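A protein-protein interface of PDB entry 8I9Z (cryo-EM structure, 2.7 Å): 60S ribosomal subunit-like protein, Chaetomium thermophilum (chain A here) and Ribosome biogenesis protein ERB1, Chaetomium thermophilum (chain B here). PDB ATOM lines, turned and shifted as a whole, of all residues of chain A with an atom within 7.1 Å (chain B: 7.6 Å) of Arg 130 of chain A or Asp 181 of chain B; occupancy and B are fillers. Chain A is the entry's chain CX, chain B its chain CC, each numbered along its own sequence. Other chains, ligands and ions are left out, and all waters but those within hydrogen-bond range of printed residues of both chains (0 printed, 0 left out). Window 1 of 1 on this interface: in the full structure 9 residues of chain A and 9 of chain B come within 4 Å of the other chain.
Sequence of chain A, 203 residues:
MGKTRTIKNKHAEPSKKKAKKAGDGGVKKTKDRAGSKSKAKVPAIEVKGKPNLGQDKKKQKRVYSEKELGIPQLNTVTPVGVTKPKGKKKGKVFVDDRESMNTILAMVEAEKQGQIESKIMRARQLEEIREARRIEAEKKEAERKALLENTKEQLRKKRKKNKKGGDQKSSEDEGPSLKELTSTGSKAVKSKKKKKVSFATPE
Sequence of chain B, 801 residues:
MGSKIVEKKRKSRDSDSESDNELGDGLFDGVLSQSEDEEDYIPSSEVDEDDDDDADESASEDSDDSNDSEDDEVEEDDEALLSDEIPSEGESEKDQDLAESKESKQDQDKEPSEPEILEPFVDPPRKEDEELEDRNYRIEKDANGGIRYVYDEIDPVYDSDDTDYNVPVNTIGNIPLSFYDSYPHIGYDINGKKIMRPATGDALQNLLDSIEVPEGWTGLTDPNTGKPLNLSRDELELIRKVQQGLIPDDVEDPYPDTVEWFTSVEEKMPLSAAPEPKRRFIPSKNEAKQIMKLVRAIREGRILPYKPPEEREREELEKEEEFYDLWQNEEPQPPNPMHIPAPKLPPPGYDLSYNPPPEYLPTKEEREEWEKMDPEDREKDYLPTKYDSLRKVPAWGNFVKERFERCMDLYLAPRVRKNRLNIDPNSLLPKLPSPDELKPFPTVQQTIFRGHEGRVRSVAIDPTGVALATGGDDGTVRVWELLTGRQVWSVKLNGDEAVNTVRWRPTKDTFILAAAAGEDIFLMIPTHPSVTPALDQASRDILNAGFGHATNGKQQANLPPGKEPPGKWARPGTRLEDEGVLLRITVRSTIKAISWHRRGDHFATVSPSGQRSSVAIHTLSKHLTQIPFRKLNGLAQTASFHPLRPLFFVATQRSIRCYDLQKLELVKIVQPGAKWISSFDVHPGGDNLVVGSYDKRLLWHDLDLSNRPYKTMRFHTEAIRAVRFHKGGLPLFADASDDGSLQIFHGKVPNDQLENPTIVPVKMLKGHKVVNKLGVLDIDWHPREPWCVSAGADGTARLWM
Among the printed residues, pairs that only touch across the chains: Leu 126 of chain A with Asp 181 of chain B (3.6 Å), Ile 129 of chain A with Ser 182 of chain B (3.8 Å), Arg 130 of chain A with Ser 182 of chain B (3.9 Å), Arg 130 of chain A with Tyr 183 of chain B (3.3 Å), Arg 130 of chain A with Pro 184 of chain B (3.5 Å), Arg 133 of chain A with Tyr 183 of chain B (3.9 Å) and Arg 133 of chain A with Pro 184 of chain B (3.9 Å).
Arg 130 of chain A touches five residues of chain B. Of chain A, only Leu 126 (3.6 Å) and Arg 130 (2.8 Å) come within 4 Å of Asp 181 of chain B. Printed residues of chain A within 4 Å of Arg 197 of chain B: Arg 130 (3.3 Å). Of the printed residues of chain A, Thr 200 of chain B touches Glu 127. Printed residues of chain A within 4 Å of Pro 184 of chain B: Arg 130 (3.5 Å) and Arg 133 (3.9 Å). His 185 of chain B touches none of the printed residues of chain A. Ala 132 of chain A touches none of the printed residues of chain B. The nearest residue of chain B that does not touch Arg 130 of chain A is Tyr 180 of chain B (4.8 Å). The nearest residue of chain A that does not touch Asp 181 of chain B is Glu 127 of chain A (5.9 Å).
Hydrophobic or aromatic side chains of chain A within 4 Å of the printed part of chain B: Leu 126 and Ile 129. Of the 16 printed residues of chain B, 6 touch a printed residue of chain A. Hydrophobic or aromatic side chains of chain B that line the printed part of chain A: Tyr 183 and Pro 184. Among the printed residues, 11 pairs touch across the chains. Among the printed residues, no Asp or Glu carboxylate lies within 4 Å of a Lys or Arg side-chain nitrogen of the other chain.
The side-chain hydroxyl (OG1) of Thr 200 of chain B lies close to the side-chain carboxylate (OE1) of Glu 127 of chain A (3.4 Å). NE of Arg 130 of chain A lies within hydrogen-bond range of O of Asp 181 of chain B, at 2.8 Å. The guanidinium group of Arg 133 of chain A is in hydrogen-bond range of the backbone carbonyl oxygen of Ser 182 of chain B (2.7 Å). The guanidinium group (NH2) of Arg 130 of chain A sits close to the guanidinium group (NH1) of Arg 197 of chain B (3.3 Å).
O of Tyr 180 of chain B lies within hydrogen-bond range of NH2 of Arg 197 of chain B (2.6 Å). The backbone carbonyl oxygen (O) of Tyr 183 of chain B lies within hydrogen-bond range of the guanidinium group (NE) of Arg 197 of chain B (3.3 Å). The backbone carbonyl oxygen of Pro 184 of chain B lies within hydrogen-bond range of the backbone NH of Arg 197 of chain B.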
ATOM      1  N   ALA A 106      27.015   7.667  -6.559  1.00  0.00           N
ATOM      2  CA  ALA A 106      25.843   8.039  -5.774  1.00  0.00           C
ATOM      3  C   ALA A 106      26.061   9.348  -5.028  1.00  0.00           C
ATOM      4  O   ALA A 106      25.140  10.163  -4.915  1.00  0.00           O
ATOM      5  CB  ALA A 106      25.489   6.918  -4.800  1.00  0.00           C
ATOM      6  N   ARG A 122      13.976  13.042  -0.310  1.00  0.00           N
ATOM      7  CA  ARG A 122      15.234  13.293   0.384  1.00  0.00           C
ATOM      8  C   ARG A 122      15.746  12.038   1.067  1.00  0.00           C
ATOM      9  O   ARG A 122      16.961  11.847   1.184  1.00  0.00           O
ATOM     10  CB  ARG A 122      15.052  14.417   1.396  1.00  0.00           C
ATOM     11  CG  ARG A 122      16.335  15.088   1.830  1.00  0.00           C
ATOM     12  CD  ARG A 122      16.304  15.473   3.323  1.00  0.00           C
ATOM     13  NE  ARG A 122      15.080  16.086   3.852  1.00  0.00           N
ATOM     14  CZ  ARG A 122      14.410  17.120   3.348  1.00  0.00           C
ATOM     15  NH1 ARG A 122      14.880  17.841   2.342  1.00  0.00           N
ATOM     16  NH2 ARG A 122      13.255  17.471   3.903  1.00  0.00           N
ATOM     17  N   ALA A 123      14.843  11.174   1.523  1.00  0.00           N
ATOM     18  CA  ALA A 123      15.261   9.916   2.125  1.00  0.00           C
ATOM     19  C   ALA A 123      15.746   8.927   1.077  1.00  0.00           C
ATOM     20  O   ALA A 123      16.740   8.228   1.299  1.00  0.00           O
ATOM     21  CB  ALA A 123      14.115   9.315   2.938  1.00  0.00           C
ATOM     22  N   GLN A 125      17.155   9.628  -1.670  1.00  0.00           N
ATOM     23  CA  GLN A 125      18.469  10.070  -2.114  1.00  0.00           C
ATOM     24  C   GLN A 125      19.571   9.547  -1.205  1.00  0.00           C
ATOM     25  O   GLN A 125      20.691   9.300  -1.664  1.00  0.00           O
ATOM     26  CB  GLN A 125      18.505  11.591  -2.178  1.00  0.00           C
ATOM     27  CG  GLN A 125      19.543  12.149  -3.107  1.00  0.00           C
ATOM     28  CD  GLN A 125      19.777  13.621  -2.873  1.00  0.00           C
ATOM     29  OE1 GLN A 125      19.855  14.074  -1.733  1.00  0.00           O
ATOM     30  NE2 GLN A 125      19.888  14.381  -3.953  1.00  0.00           N
ATOM     31  N   LEU A 126      19.275   9.362   0.078  1.00  0.00           N
ATOM     32  CA  LEU A 126      20.232   8.823   1.032  1.00  0.00           C
ATOM     33  C   LEU A 126      20.253   7.303   1.055  1.00  0.00           C
ATOM     34  O   LEU A 126      21.314   6.713   1.271  1.00  0.00           O
ATOM     35  CB  LEU A 126      19.930   9.337   2.441  1.00  0.00           C
ATOM     36  CG  LEU A 126      20.365  10.759   2.782  1.00  0.00           C
ATOM     37  CD1 LEU A 126      19.868  11.135   4.162  1.00  0.00           C
ATOM     38  CD2 LEU A 126      21.873  10.888   2.703  1.00  0.00           C
ATOM     39  N   GLU A 127      19.105   6.653   0.846  1.00  0.00           N
ATOM     40  CA  GLU A 127      19.076   5.194   0.850  1.00  0.00           C
ATOM     41  C   GLU A 127      19.788   4.613  -0.361  1.00  0.00           C
ATOM     42  O   GLU A 127      20.274   3.478  -0.307  1.00  0.00           O
ATOM     43  CB  GLU A 127      17.636   4.693   0.904  1.00  0.00           C
ATOM     44  CG  GLU A 127      16.880   5.099   2.151  1.00  0.00           C
ATOM     45  CD  GLU A 127      15.838   4.077   2.551  1.00  0.00           C
ATOM     46  OE1 GLU A 127      14.997   3.722   1.698  1.00  0.00           O
ATOM     47  OE2 GLU A 127      15.858   3.630   3.717  1.00  0.00           O
ATOM     48  N   GLU A 128      19.843   5.360  -1.463  1.00  0.00           N
ATOM     49  CA  GLU A 128      20.601   4.914  -2.625  1.00  0.00           C
ATOM     50  C   GLU A 128      22.092   4.882  -2.323  1.00  0.00           C
ATOM     51  O   GLU A 128      22.810   3.980  -2.767  1.00  0.00           O
ATOM     52  CB  GLU A 128      20.306   5.821  -3.817  1.00  0.00           C
ATOM     53  CG  GLU A 128      19.164   5.334  -4.690  1.00  0.00           C
ATOM     54  CD  GLU A 128      19.129   6.021  -6.041  1.00  0.00           C
ATOM     55  OE1 GLU A 128      19.750   7.096  -6.179  1.00  0.00           O
ATOM     56  OE2 GLU A 128      18.482   5.484  -6.966  1.00  0.00           O
ATOM     57  N   ILE A 129      22.576   5.870  -1.571  1.00  0.00           N
ATOM     58  CA  ILE A 129      23.975   5.884  -1.163  1.00  0.00           C
ATOM     59  C   ILE A 129      24.243   4.787  -0.142  1.00  0.00           C
ATOM     60  O   ILE A 129      25.303   4.148  -0.159  1.00  0.00           O
ATOM     61  CB  ILE A 129      24.355   7.274  -0.625  1.00  0.00           C
ATOM     62  CG1 ILE A 129      23.978   8.352  -1.639  1.00  0.00           C
ATOM     63  CG2 ILE A 129      25.838   7.351  -0.323  1.00  0.00           C
ATOM     64  CD1 ILE A 129      24.353   9.738  -1.210  1.00  0.00           C
ATOM     65  N   ARG A 130      23.291   4.551   0.766  1.00  0.00           N
ATOM     66  CA  ARG A 130      23.461   3.509   1.775  1.00  0.00           C
ATOM     67  C   ARG A 130      23.498   2.118   1.153  1.00  0.00           C
ATOM     68  O   ARG A 130      24.316   1.279   1.543  1.00  0.00           O
ATOM     69  CB  ARG A 130      22.342   3.585   2.811  1.00  0.00           C
ATOM     70  CG  ARG A 130      22.414   4.769   3.739  1.00  0.00           C
ATOM     71  CD  ARG A 130      21.197   4.815   4.638  1.00  0.00           C
ATOM     72  NE  ARG A 130      20.948   6.154   5.154  1.00  0.00           N
ATOM     73  CZ  ARG A 130      19.772   6.580   5.590  1.00  0.00           C
ATOM     74  NH1 ARG A 130      18.714   5.789   5.600  1.00  0.00           N
ATOM     75  NH2 ARG A 130      19.655   7.831   6.022  1.00  0.00           N
ATOM     76  N   GLU A 131      22.607   1.849   0.196  1.00  0.00           N
ATOM     77  CA  GLU A 131      22.587   0.537  -0.442  1.00  0.00           C
ATOM     78  C   GLU A 131      23.815   0.330  -1.312  1.00  0.00           C
ATOM     79  O   GLU A 131      24.285  -0.802  -1.471  1.00  0.00           O
ATOM     80  CB  GLU A 131      21.315   0.369  -1.270  1.00  0.00           C
ATOM     81  CG  GLU A 131      20.244  -0.472  -0.605  1.00  0.00           C
ATOM     82  CD  GLU A 131      18.885  -0.304  -1.259  1.00  0.00           C
ATOM     83  OE1 GLU A 131      18.838   0.095  -2.442  1.00  0.00           O
ATOM     84  OE2 GLU A 131      17.865  -0.572  -0.590  1.00  0.00           O
ATOM     85  N   ALA A 132      24.341   1.408  -1.890  1.00  0.00           N
ATOM     86  CA  ALA A 132      25.564   1.308  -2.676  1.00  0.00           C
ATOM     87  C   ALA A 132      26.756   0.968  -1.792  1.00  0.00           C
ATOM     88  O   ALA A 132      27.672   0.254  -2.213  1.00  0.00           O
ATOM     89  CB  ALA A 132      25.806   2.611  -3.434  1.00  0.00           C
ATOM     90  N   ARG A 133      26.765   1.482  -0.563  1.00  0.00           N
ATOM     91  CA  ARG A 133      27.851   1.170   0.357  1.00  0.00           C
ATOM     92  C   ARG A 133      27.770  -0.268   0.844  1.00  0.00           C
ATOM     93  O   ARG A 133      28.799  -0.913   1.072  1.00  0.00           O
ATOM     94  CB  ARG A 133      27.829   2.132   1.540  1.00  0.00           C
ATOM     95  CG  ARG A 133      28.321   3.529   1.231  1.00  0.00           C
ATOM     96  CD  ARG A 133      28.601   4.281   2.511  1.00  0.00           C
ATOM     97  NE  ARG A 133      28.618   5.723   2.319  1.00  0.00           N
ATOM     98  CZ  ARG A 133      29.715   6.441   2.127  1.00  0.00           C
ATOM     99  NH1 ARG A 133      30.909   5.877   2.077  1.00  0.00           N
ATOM    100  NH2 ARG A 133      29.610   7.757   1.983  1.00  0.00           N
ATOM    101  N   ARG A 134      26.554  -0.786   1.020  1.00  0.00           N
ATOM    102  CA  ARG A 134      26.387  -2.143   1.529  1.00  0.00           C
ATOM    103  C   ARG A 134      26.799  -3.179   0.494  1.00  0.00           C
ATOM    104  O   ARG A 134      27.451  -4.176   0.822  1.00  0.00           O
ATOM    105  CB  ARG A 134      24.939  -2.364   1.958  1.00  0.00           C
ATOM    106  CG  ARG A 134      24.686  -3.694   2.635  1.00  0.00           C
ATOM    107  CD  ARG A 134      23.183  -3.982   2.747  1.00  0.00           C
ATOM    108  NE  ARG A 134      22.447  -4.362   1.536  1.00  0.00           N
ATOM    109  CZ  ARG A 134      22.828  -5.184   0.560  1.00  0.00           C
ATOM    110  NH1 ARG A 134      23.884  -5.975   0.671  1.00  0.00           N
ATOM    111  NH2 ARG A 134      22.084  -5.266  -0.539  1.00  0.00           N
ATOM    112  N   ILE A 135      26.409  -2.967  -0.764  1.00  0.00           N
ATOM    113  CA  ILE A 135      26.743  -3.912  -1.823  1.00  0.00           C
ATOM    114  C   ILE A 135      28.245  -3.919  -2.075  1.00  0.00           C
ATOM    115  O   ILE A 135      28.845  -4.975  -2.304  1.00  0.00           O
ATOM    116  CB  ILE A 135      25.941  -3.576  -3.094  1.00  0.00           C
ATOM    117  CG1 ILE A 135      24.449  -3.768  -2.837  1.00  0.00           C
ATOM    118  CG2 ILE A 135      26.368  -4.441  -4.262  1.00  0.00           C
ATOM    119  CD1 ILE A 135      23.567  -3.206  -3.922  1.00  0.00           C
ATOM    120  N   GLU A 136      28.879  -2.750  -2.007  1.00  0.00           N
ATOM    121  CA  GLU A 136      30.327  -2.677  -2.170  1.00  0.00           C
ATOM    122  C   GLU A 136      31.050  -3.358  -1.016  1.00  0.00           C
ATOM    123  O   GLU A 136      32.094  -3.991  -1.215  1.00  0.00           O
ATOM    124  CB  GLU A 136      30.763  -1.220  -2.289  1.00  0.00           C
ATOM    125  CG  GLU A 136      32.217  -1.027  -2.643  1.00  0.00           C
ATOM    126  CD  GLU A 136      32.789   0.244  -2.053  1.00  0.00           C
ATOM    127  OE1 GLU A 136      32.047   0.960  -1.352  1.00  0.00           O
ATOM    128  OE2 GLU A 136      33.982   0.528  -2.291  1.00  0.00           O
ATOM    129  N   PRO B 176      25.854  15.652  16.280  1.00  0.00           N
ATOM    130  CA  PRO B 176      24.685  15.525  15.404  1.00  0.00           C
ATOM    131  C   PRO B 176      24.702  14.210  14.642  1.00  0.00           C
ATOM    132  O   PRO B 176      25.756  13.623  14.390  1.00  0.00           O
ATOM    133  CB  PRO B 176      24.817  16.719  14.453  1.00  0.00           C
ATOM    134  CG  PRO B 176      26.229  17.161  14.566  1.00  0.00           C
ATOM    135  CD  PRO B 176      26.675  16.825  15.944  1.00  0.00           C
ATOM    136  N   LEU B 177      23.510  13.750  14.267  1.00  0.00           N
ATOM    137  CA  LEU B 177      23.356  12.467  13.596  1.00  0.00           C
ATOM    138  C   LEU B 177      23.425  12.582  12.081  1.00  0.00           C
ATOM    139  O   LEU B 177      23.130  11.611  11.373  1.00  0.00           O
ATOM    140  CB  LEU B 177      22.047  11.809  14.016  1.00  0.00           C
ATOM    141  CG  LEU B 177      22.245  10.736  15.074  1.00  0.00           C
ATOM    142  CD1 LEU B 177      20.922  10.418  15.736  1.00  0.00           C
ATOM    143  CD2 LEU B 177      22.890   9.510  14.475  1.00  0.00           C
ATOM    144  N   SER B 178      23.812  13.742  11.562  1.00  0.00           N
ATOM    145  CA  SER B 178      24.007  13.930  10.136  1.00  0.00           C
ATOM    146  C   SER B 178      25.345  13.390   9.655  1.00  0.00           C
ATOM    147  O   SER B 178      25.597  13.380   8.448  1.00  0.00           O
ATOM    148  CB  SER B 178      23.887  15.413   9.779  1.00  0.00           C
ATOM    149  OG  SER B 178      24.884  16.175  10.431  1.00  0.00           O
ATOM    150  N   PHE B 179      26.206  12.948  10.565  1.00  0.00           N
ATOM    151  CA  PHE B 179      27.448  12.290  10.201  1.00  0.00           C
ATOM    152  C   PHE B 179      27.227  10.873   9.699  1.00  0.00           C
ATOM    153  O   PHE B 179      28.101  10.327   9.021  1.00  0.00           O
ATOM    154  CB  PHE B 179      28.401  12.264  11.399  1.00  0.00           C
ATOM    155  CG  PHE B 179      29.039  13.584  11.685  1.00  0.00           C
ATOM    156  CD1 PHE B 179      30.151  13.995  10.979  1.00  0.00           C
ATOM    157  CD2 PHE B 179      28.527  14.413  12.662  1.00  0.00           C
ATOM    158  CE1 PHE B 179      30.738  15.210  11.240  1.00  0.00           C
ATOM    159  CE2 PHE B 179      29.109  15.630  12.925  1.00  0.00           C
ATOM    160  CZ  PHE B 179      30.216  16.028  12.214  1.00  0.00           C
ATOM    161  N   TYR B 180      26.080  10.277  10.008  1.00  0.00           N
ATOM    162  CA  TYR B 180      25.755   8.928   9.586  1.00  0.00           C
ATOM    163  C   TYR B 180      24.670   8.886   8.527  1.00  0.00           C
ATOM    164  O   TYR B 180      24.066   7.826   8.332  1.00  0.00           O
ATOM    165  CB  TYR B 180      25.294   8.092  10.785  1.00  0.00           C
ATOM    166  CG  TYR B 180      26.371   7.760  11.782  1.00  0.00           C
ATOM    167  CD1 TYR B 180      27.316   6.782  11.519  1.00  0.00           C
ATOM    168  CD2 TYR B 180      26.431   8.416  12.998  1.00  0.00           C
ATOM    169  CE1 TYR B 180      28.294   6.478  12.437  1.00  0.00           C
ATOM    170  CE2 TYR B 180      27.404   8.118  13.918  1.00  0.00           C
ATOM    171  CZ  TYR B 180      28.330   7.150  13.633  1.00  0.00           C
ATOM    172  OH  TYR B 180      29.300   6.857  14.555  1.00  0.00           O
ATOM    173  N   ASP B 181      24.388  10.005   7.859  1.00  0.00           N
ATOM    174  CA  ASP B 181      23.241  10.082   6.959  1.00  0.00           C
ATOM    175  C   ASP B 181      23.412   9.168   5.754  1.00  0.00           C
ATOM    176  O   ASP B 181      22.460   8.515   5.313  1.00  0.00           O
ATOM    177  CB  ASP B 181      23.030  11.527   6.510  1.00  0.00           C
ATOM    178  CG  ASP B 181      22.103  12.294   7.430  1.00  0.00           C
ATOM    179  OD1 ASP B 181      21.947  13.516   7.232  1.00  0.00           O
ATOM    180  OD2 ASP B 181      21.533  11.675   8.353  1.00  0.00           O
ATOM    181  N   SER B 182      24.623   9.107   5.209  1.00  0.00           N
ATOM    182  CA  SER B 182      24.900   8.316   4.019  1.00  0.00           C
ATOM    183  C   SER B 182      25.520   6.966   4.338  1.00  0.00           C
ATOM    184  O   SER B 182      26.277   6.432   3.519  1.00  0.00           O
ATOM    185  CB  SER B 182      25.805   9.101   3.073  1.00  0.00           C
ATOM    186  OG  SER B 182      27.098   9.258   3.627  1.00  0.00           O
ATOM    187  N   TYR B 183      25.216   6.387   5.494  1.00  0.00           N
ATOM    188  CA  TYR B 183      25.862   5.143   5.870  1.00  0.00           C
ATOM    189  C   TYR B 183      24.837   4.079   6.232  1.00  0.00           C
ATOM    190  O   TYR B 183      23.761   4.400   6.747  1.00  0.00           O
ATOM    191  CB  TYR B 183      26.814   5.361   7.050  1.00  0.00           C
ATOM    192  CG  TYR B 183      28.093   6.051   6.662  1.00  0.00           C
ATOM    193  CD1 TYR B 183      28.176   7.431   6.626  1.00  0.00           C
ATOM    194  CD2 TYR B 183      29.213   5.319   6.315  1.00  0.00           C
ATOM    195  CE1 TYR B 183      29.343   8.061   6.265  1.00  0.00           C
ATOM    196  CE2 TYR B 183      30.381   5.936   5.956  1.00  0.00           C
ATOM    197  CZ  TYR B 183      30.444   7.305   5.932  1.00  0.00           C
ATOM    198  OH  TYR B 183      31.613   7.926   5.569  1.00  0.00           O
ATOM    199  N   PRO B 184      25.132   2.804   5.966  1.00  0.00           N
ATOM    200  CA  PRO B 184      24.193   1.744   6.349  1.00  0.00           C
ATOM    201  C   PRO B 184      24.097   1.539   7.846  1.00  0.00           C
ATOM    202  O   PRO B 184      23.091   0.998   8.315  1.00  0.00           O
ATOM    203  CB  PRO B 184      24.763   0.496   5.659  1.00  0.00           C
ATOM    204  CG  PRO B 184      25.812   0.986   4.733  1.00  0.00           C
ATOM    205  CD  PRO B 184      26.323   2.251   5.306  1.00  0.00           C
ATOM    206  N   HIS B 185      25.104   1.947   8.607  1.00  0.00           N
ATOM    207  CA  HIS B 185      25.151   1.733  10.042  1.00  0.00           C
ATOM    208  C   HIS B 185      24.925   3.047  10.773  1.00  0.00           C
ATOM    209  O   HIS B 185      25.020   4.131  10.196  1.00  0.00           O
ATOM    210  CB  HIS B 185      26.492   1.124  10.468  1.00  0.00           C
ATOM    211  CG  HIS B 185      27.671   1.992  10.162  1.00  0.00           C
ATOM    212  ND1 HIS B 185      28.076   3.020  10.982  1.00  0.00           N
ATOM    213  CD2 HIS B 185      28.525   1.992   9.112  1.00  0.00           C
ATOM    214  CE1 HIS B 185      29.129   3.614  10.452  1.00  0.00           C
ATOM    215  NE2 HIS B 185      29.422   3.008   9.318  1.00  0.00           N
ATOM    216  N   ILE B 186      24.625   2.929  12.060  1.00  0.00           N
ATOM    217  CA  ILE B 186      24.448   4.080  12.941  1.00  0.00           C
ATOM    218  C   ILE B 186      25.177   3.776  14.254  1.00  0.00           C
ATOM    219  O   ILE B 186      24.712   3.012  15.105  1.00  0.00           O
ATOM    220  CB  ILE B 186      22.963   4.460  13.116  1.00  0.00           C
ATOM    221  CG1 ILE B 186      22.774   5.921  13.536  1.00  0.00           C
ATOM    222  CG2 ILE B 186      22.039   3.400  13.794  1.00  0.00           C
ATOM    223  CD1 ILE B 186      21.342   6.248  13.904  1.00  0.00           C
ATOM    224  N   ARG B 197      21.277  -0.037  10.783  1.00  0.00           N
ATOM    225  CA  ARG B 197      19.964   0.585  10.734  1.00  0.00           C
ATOM    226  C   ARG B 197      18.897  -0.494  10.577  1.00  0.00           C
ATOM    227  O   ARG B 197      19.116  -1.478   9.863  1.00  0.00           O
ATOM    228  CB  ARG B 197      19.879   1.589   9.588  1.00  0.00           C
ATOM    229  CG  ARG B 197      20.755   2.798   9.771  1.00  0.00           C
ATOM    230  CD  ARG B 197      20.483   3.797   8.689  1.00  0.00           C
ATOM    231  NE  ARG B 197      21.300   4.993   8.811  1.00  0.00           N
ATOM    232  CZ  ARG B 197      20.810   6.212   8.958  1.00  0.00           C
ATOM    233  NH1 ARG B 197      19.510   6.425   9.056  1.00  0.00           N
ATOM    234  NH2 ARG B 197      21.643   7.245   9.007  1.00  0.00           N
ATOM    235  N   ALA B 199      15.493  -0.970   9.340  1.00  0.00           N
ATOM    236  CA  ALA B 199      14.756  -1.245   8.109  1.00  0.00           C
ATOM    237  C   ALA B 199      14.312   0.095   7.538  1.00  0.00           C
ATOM    238  O   ALA B 199      14.724   1.160   8.015  1.00  0.00           O
ATOM    239  CB  ALA B 199      13.562  -2.170   8.352  1.00  0.00           C
ATOM    240  N   THR B 200      13.465   0.043   6.517  1.00  0.00           N
ATOM    241  CA  THR B 200      12.920   1.234   5.884  1.00  0.00           C
ATOM    242  C   THR B 200      11.403   1.141   5.908  1.00  0.00           C
ATOM    243  O   THR B 200      10.830   0.168   5.402  1.00  0.00           O
ATOM    244  CB  THR B 200      13.430   1.373   4.449  1.00  0.00           C
ATOM    245  OG1 THR B 200      14.830   1.674   4.469  1.00  0.00           O
ATOM    246  CG2 THR B 200      12.687   2.482   3.722  1.00  0.00           C
ATOM    247  N   THR B 221      14.989  12.207  16.001  1.00  0.00           N
ATOM    248  CA  THR B 221      15.525  10.944  15.523  1.00  0.00           C
ATOM    249  C   THR B 221      16.197  10.225  16.681  1.00  0.00           C
ATOM    250  O   THR B 221      17.003  10.822  17.401  1.00  0.00           O
ATOM    251  CB  THR B 221      16.522  11.164  14.385  1.00  0.00           C
ATOM    252  OG1 THR B 221      15.957  12.049  13.412  1.00  0.00           O
ATOM    253  CG2 THR B 221      16.869   9.846  13.717  1.00  0.00           C
ATOM    254  N   GLY B 226      17.687   4.825  13.395  1.00  0.00           N
ATOM    255  CA  GLY B 226      17.404   6.043  12.655  1.00  0.00           C
ATOM    256  C   GLY B 226      15.936   6.361  12.426  1.00  0.00           C
ATOM    257  O   GLY B 226      15.613   7.403  11.851  1.00  0.00           O
